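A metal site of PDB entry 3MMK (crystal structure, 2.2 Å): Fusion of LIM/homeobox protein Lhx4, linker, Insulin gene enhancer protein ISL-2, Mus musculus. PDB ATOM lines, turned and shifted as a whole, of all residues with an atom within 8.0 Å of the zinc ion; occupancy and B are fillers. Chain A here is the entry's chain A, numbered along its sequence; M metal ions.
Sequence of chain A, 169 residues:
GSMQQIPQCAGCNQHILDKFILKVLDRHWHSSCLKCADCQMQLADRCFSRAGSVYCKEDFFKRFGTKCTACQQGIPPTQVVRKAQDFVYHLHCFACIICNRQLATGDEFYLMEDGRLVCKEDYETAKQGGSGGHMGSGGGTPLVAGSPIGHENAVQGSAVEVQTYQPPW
The zinc ion is bound by ND1 of His 90 (2.2 Å), SG of Cys 93 (2.4 Å), SG of Cys 68 (2.4 Å) and SG of Cys 71 (2.4 Å). The zinc ion has four donor atoms within binding distance.
The side-chain sulfur (SG) of Cys 93 lies close to a ring nitrogen (ND1) of His 92 (3.5 Å). N of Cys 68 lies within hydrogen-bond range of O of Gln 73, at 2.9 Å. N of Ala 70 lies close to SG of Cys 68, 3.5 Å away. The side-chain sulfur (SG) of Cys 71 sits close to the side-chain amide oxygen (OE1) of Gln 73, 3.7 Å away. A ring nitrogen (NE2) of His 90 sits at hydrogen-bond distance from the backbone carbonyl oxygen of Gly 74 (3.2 Å).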
ATOM      1  N   LYS A  67     -22.903 -36.811  18.455  1.00  0.00           N
ATOM      2  CA  LYS A  67     -21.901 -35.962  17.840  1.00  0.00           C
ATOM      3  C   LYS A  67     -22.400 -34.533  17.686  1.00  0.00           C
ATOM      4  O   LYS A  67     -23.509 -34.303  17.207  1.00  0.00           O
ATOM      5  CB  LYS A  67     -21.503 -36.531  16.476  1.00  0.00           C
ATOM      6  N   CYS A  68     -21.576 -33.569  18.085  1.00  0.00           N
ATOM      7  CA  CYS A  68     -21.943 -32.167  17.981  1.00  0.00           C
ATOM      8  C   CYS A  68     -22.186 -31.763  16.530  1.00  0.00           C
ATOM      9  O   CYS A  68     -21.424 -32.120  15.647  1.00  0.00           O
ATOM     10  CB  CYS A  68     -20.867 -31.274  18.598  1.00  0.00           C
ATOM     11  SG  CYS A  68     -21.205 -29.504  18.413  1.00  0.00           S
ATOM     12  N   THR A  69     -23.253 -31.010  16.307  1.00  0.00           N
ATOM     13  CA  THR A  69     -23.652 -30.614  14.961  1.00  0.00           C
ATOM     14  C   THR A  69     -22.582 -29.772  14.283  1.00  0.00           C
ATOM     15  O   THR A  69     -22.320 -29.930  13.095  1.00  0.00           O
ATOM     16  CB  THR A  69     -24.971 -29.827  14.988  1.00  0.00           C
ATOM     17  OG1 THR A  69     -26.023 -30.678  15.460  1.00  0.00           O
ATOM     18  CG2 THR A  69     -25.308 -29.304  13.605  1.00  0.00           C
ATOM     19  N   ALA A  70     -21.975 -28.866  15.040  1.00  0.00           N
ATOM     20  CA  ALA A  70     -20.996 -27.928  14.485  1.00  0.00           C
ATOM     21  C   ALA A  70     -19.644 -28.580  14.191  1.00  0.00           C
ATOM     22  O   ALA A  70     -19.100 -28.430  13.104  1.00  0.00           O
ATOM     23  CB  ALA A  70     -20.828 -26.723  15.411  1.00  0.00           C
ATOM     24  N   CYS A  71     -19.108 -29.303  15.174  1.00  0.00           N
ATOM     25  CA  CYS A  71     -17.750 -29.858  15.049  1.00  0.00           C
ATOM     26  C   CYS A  71     -17.755 -31.353  14.757  1.00  0.00           C
ATOM     27  O   CYS A  71     -16.701 -31.935  14.492  1.00  0.00           O
ATOM     28  CB  CYS A  71     -16.937 -29.568  16.309  1.00  0.00           C
ATOM     29  SG  CYS A  71     -17.299 -30.655  17.714  1.00  0.00           S
ATOM     30  N   GLN A  72     -18.927 -31.980  14.820  1.00  0.00           N
ATOM     31  CA  GLN A  72     -19.072 -33.398  14.514  1.00  0.00           C
ATOM     32  C   GLN A  72     -18.194 -34.290  15.377  1.00  0.00           C
ATOM     33  O   GLN A  72     -17.500 -35.176  14.876  1.00  0.00           O
ATOM     34  CB  GLN A  72     -18.797 -33.650  13.030  1.00  0.00           C
ATOM     35  CG  GLN A  72     -19.816 -33.024  12.095  1.00  0.00           C
ATOM     36  CD  GLN A  72     -19.406 -33.083  10.635  1.00  0.00           C
ATOM     37  OE1 GLN A  72     -18.273 -33.444  10.316  1.00  0.00           O
ATOM     38  NE2 GLN A  72     -20.329 -32.749   9.746  1.00  0.00           N
ATOM     39  N   GLN A  73     -18.237 -34.069  16.689  1.00  0.00           N
ATOM     40  CA  GLN A  73     -17.462 -34.857  17.636  1.00  0.00           C
ATOM     41  C   GLN A  73     -18.231 -35.161  18.913  1.00  0.00           C
ATOM     42  O   GLN A  73     -19.105 -34.393  19.322  1.00  0.00           O
ATOM     43  CB  GLN A  73     -16.143 -34.155  17.965  1.00  0.00           C
ATOM     44  CG  GLN A  73     -15.173 -34.087  16.794  1.00  0.00           C
ATOM     45  CD  GLN A  73     -13.973 -33.223  17.086  1.00  0.00           C
ATOM     46  OE1 GLN A  73     -14.036 -32.295  17.899  1.00  0.00           O
ATOM     47  NE2 GLN A  73     -12.856 -33.519  16.421  1.00  0.00           N
ATOM     48  N   GLY A  74     -17.916 -36.291  19.541  1.00  0.00           N
ATOM     49  CA  GLY A  74     -18.653 -36.770  20.697  1.00  0.00           C
ATOM     50  C   GLY A  74     -18.728 -35.808  21.859  1.00  0.00           C
ATOM     51  O   GLY A  74     -17.885 -34.925  22.026  1.00  0.00           O
ATOM     52  N   ILE A  75     -19.769 -35.981  22.676  1.00  0.00           N
ATOM     53  CA  ILE A  75     -19.996 -35.135  23.839  1.00  0.00           C
ATOM     54  C   ILE A  75     -20.377 -35.967  25.055  1.00  0.00           C
ATOM     55  O   ILE A  75     -19.566 -36.743  25.575  1.00  0.00           O
ATOM     56  CB  ILE A  75     -21.112 -34.107  23.568  1.00  0.00           C
ATOM     57  CG1 ILE A  75     -22.413 -34.823  23.196  1.00  0.00           C
ATOM     58  CG2 ILE A  75     -20.725 -33.169  22.449  1.00  0.00           C
ATOM     59  CD1 ILE A  75     -23.411 -33.929  22.505  1.00  0.00           C
ATOM     60  N   VAL A  88     -27.846 -30.716  18.135  1.00  0.00           N
ATOM     61  CA  VAL A  88     -27.227 -30.776  19.458  1.00  0.00           C
ATOM     62  C   VAL A  88     -25.782 -30.243  19.387  1.00  0.00           C
ATOM     63  O   VAL A  88     -25.056 -30.552  18.444  1.00  0.00           O
ATOM     64  CB  VAL A  88     -27.225 -32.215  20.004  1.00  0.00           C
ATOM     65  CG1 VAL A  88     -26.818 -32.217  21.469  1.00  0.00           C
ATOM     66  CG2 VAL A  88     -28.598 -32.839  19.853  1.00  0.00           C
ATOM     67  N   TYR A  89     -25.383 -29.465  20.383  1.00  0.00           N
ATOM     68  CA  TYR A  89     -24.081 -28.796  20.358  1.00  0.00           C
ATOM     69  C   TYR A  89     -23.333 -28.852  21.681  1.00  0.00           C
ATOM     70  O   TYR A  89     -23.945 -28.866  22.748  1.00  0.00           O
ATOM     71  CB  TYR A  89     -24.252 -27.318  19.993  1.00  0.00           C
ATOM     72  CG  TYR A  89     -25.094 -27.034  18.764  1.00  0.00           C
ATOM     73  CD1 TYR A  89     -26.479 -27.053  18.822  1.00  0.00           C
ATOM     74  CD2 TYR A  89     -24.492 -26.708  17.560  1.00  0.00           C
ATOM     75  CE1 TYR A  89     -27.236 -26.781  17.707  1.00  0.00           C
ATOM     76  CE2 TYR A  89     -25.246 -26.428  16.433  1.00  0.00           C
ATOM     77  CZ  TYR A  89     -26.612 -26.463  16.509  1.00  0.00           C
ATOM     78  OH  TYR A  89     -27.368 -26.191  15.394  1.00  0.00           O
ATOM     79  N   HIS A  90     -22.006 -28.879  21.598  1.00  0.00           N
ATOM     80  CA  HIS A  90     -21.160 -28.510  22.736  1.00  0.00           C
ATOM     81  C   HIS A  90     -21.576 -27.094  23.128  1.00  0.00           C
ATOM     82  O   HIS A  90     -22.007 -26.324  22.278  1.00  0.00           O
ATOM     83  CB  HIS A  90     -19.687 -28.461  22.337  1.00  0.00           C
ATOM     84  CG  HIS A  90     -19.047 -29.803  22.156  1.00  0.00           C
ATOM     85  ND1 HIS A  90     -18.898 -30.389  20.910  1.00  0.00           N
ATOM     86  CD2 HIS A  90     -18.504 -30.667  23.048  1.00  0.00           C
ATOM     87  CE1 HIS A  90     -18.295 -31.566  21.054  1.00  0.00           C
ATOM     88  NE2 HIS A  90     -18.049 -31.748  22.340  1.00  0.00           N
ATOM     89  N   LEU A  91     -21.439 -26.761  24.405  1.00  0.00           N
ATOM     90  CA  LEU A  91     -21.722 -25.409  24.846  1.00  0.00           C
ATOM     91  C   LEU A  91     -20.814 -24.405  24.123  1.00  0.00           C
ATOM     92  O   LEU A  91     -21.246 -23.314  23.754  1.00  0.00           O
ATOM     93  CB  LEU A  91     -21.560 -25.273  26.366  1.00  0.00           C
ATOM     94  CG  LEU A  91     -22.794 -25.581  27.206  1.00  0.00           C
ATOM     95  CD1 LEU A  91     -23.371 -26.961  26.870  1.00  0.00           C
ATOM     96  CD2 LEU A  91     -22.468 -25.477  28.688  1.00  0.00           C
ATOM     97  N   HIS A  92     -19.562 -24.789  23.916  1.00  0.00           N
ATOM     98  CA  HIS A  92     -18.597 -23.903  23.276  1.00  0.00           C
ATOM     99  C   HIS A  92     -18.765 -23.866  21.758  1.00  0.00           C
ATOM    100  O   HIS A  92     -18.177 -23.020  21.088  1.00  0.00           O
ATOM    101  CB  HIS A  92     -17.160 -24.289  23.624  1.00  0.00           C
ATOM    102  CG  HIS A  92     -16.846 -25.740  23.417  1.00  0.00           C
ATOM    103  ND1 HIS A  92     -16.460 -26.247  22.185  1.00  0.00           N
ATOM    104  CD2 HIS A  92     -16.854 -26.789  24.272  1.00  0.00           C
ATOM    105  CE1 HIS A  92     -16.242 -27.544  22.301  1.00  0.00           C
ATOM    106  NE2 HIS A  92     -16.475 -27.897  23.557  1.00  0.00           N
ATOM    107  N   CYS A  93     -19.583 -24.777  21.222  1.00  0.00           N
ATOM    108  CA  CYS A  93     -19.888 -24.783  19.797  1.00  0.00           C
ATOM    109  C   CYS A  93     -21.213 -24.111  19.509  1.00  0.00           C
ATOM    110  O   CYS A  93     -21.508 -23.774  18.362  1.00  0.00           O
ATOM    111  CB  CYS A  93     -19.888 -26.210  19.246  1.00  0.00           C
ATOM    112  SG  CYS A  93     -18.253 -26.963  19.277  1.00  0.00           S
ATOM    113  N   PHE A  94     -22.013 -23.912  20.554  1.00  0.00           N
ATOM    114  CA  PHE A  94     -23.248 -23.149  20.438  1.00  0.00           C
ATOM    115  C   PHE A  94     -22.861 -21.679  20.316  1.00  0.00           C
ATOM    116  O   PHE A  94     -23.023 -20.910  21.269  1.00  0.00           O
ATOM    117  CB  PHE A  94     -24.105 -23.383  21.687  1.00  0.00           C
ATOM    118  CG  PHE A  94     -25.558 -23.085  21.484  1.00  0.00           C
ATOM    119  CD1 PHE A  94     -26.291 -23.751  20.506  1.00  0.00           C
ATOM    120  CD2 PHE A  94     -26.218 -22.167  22.290  1.00  0.00           C
ATOM    121  CE1 PHE A  94     -27.639 -23.490  20.331  1.00  0.00           C
ATOM    122  CE2 PHE A  94     -27.566 -21.907  22.115  1.00  0.00           C
ATOM    123  CZ  PHE A  94     -28.275 -22.572  21.133  1.00  0.00           C
HETATM  124 ZN    ZN M   1     -18.857 -29.259  18.970  1.00  0.00          ZN
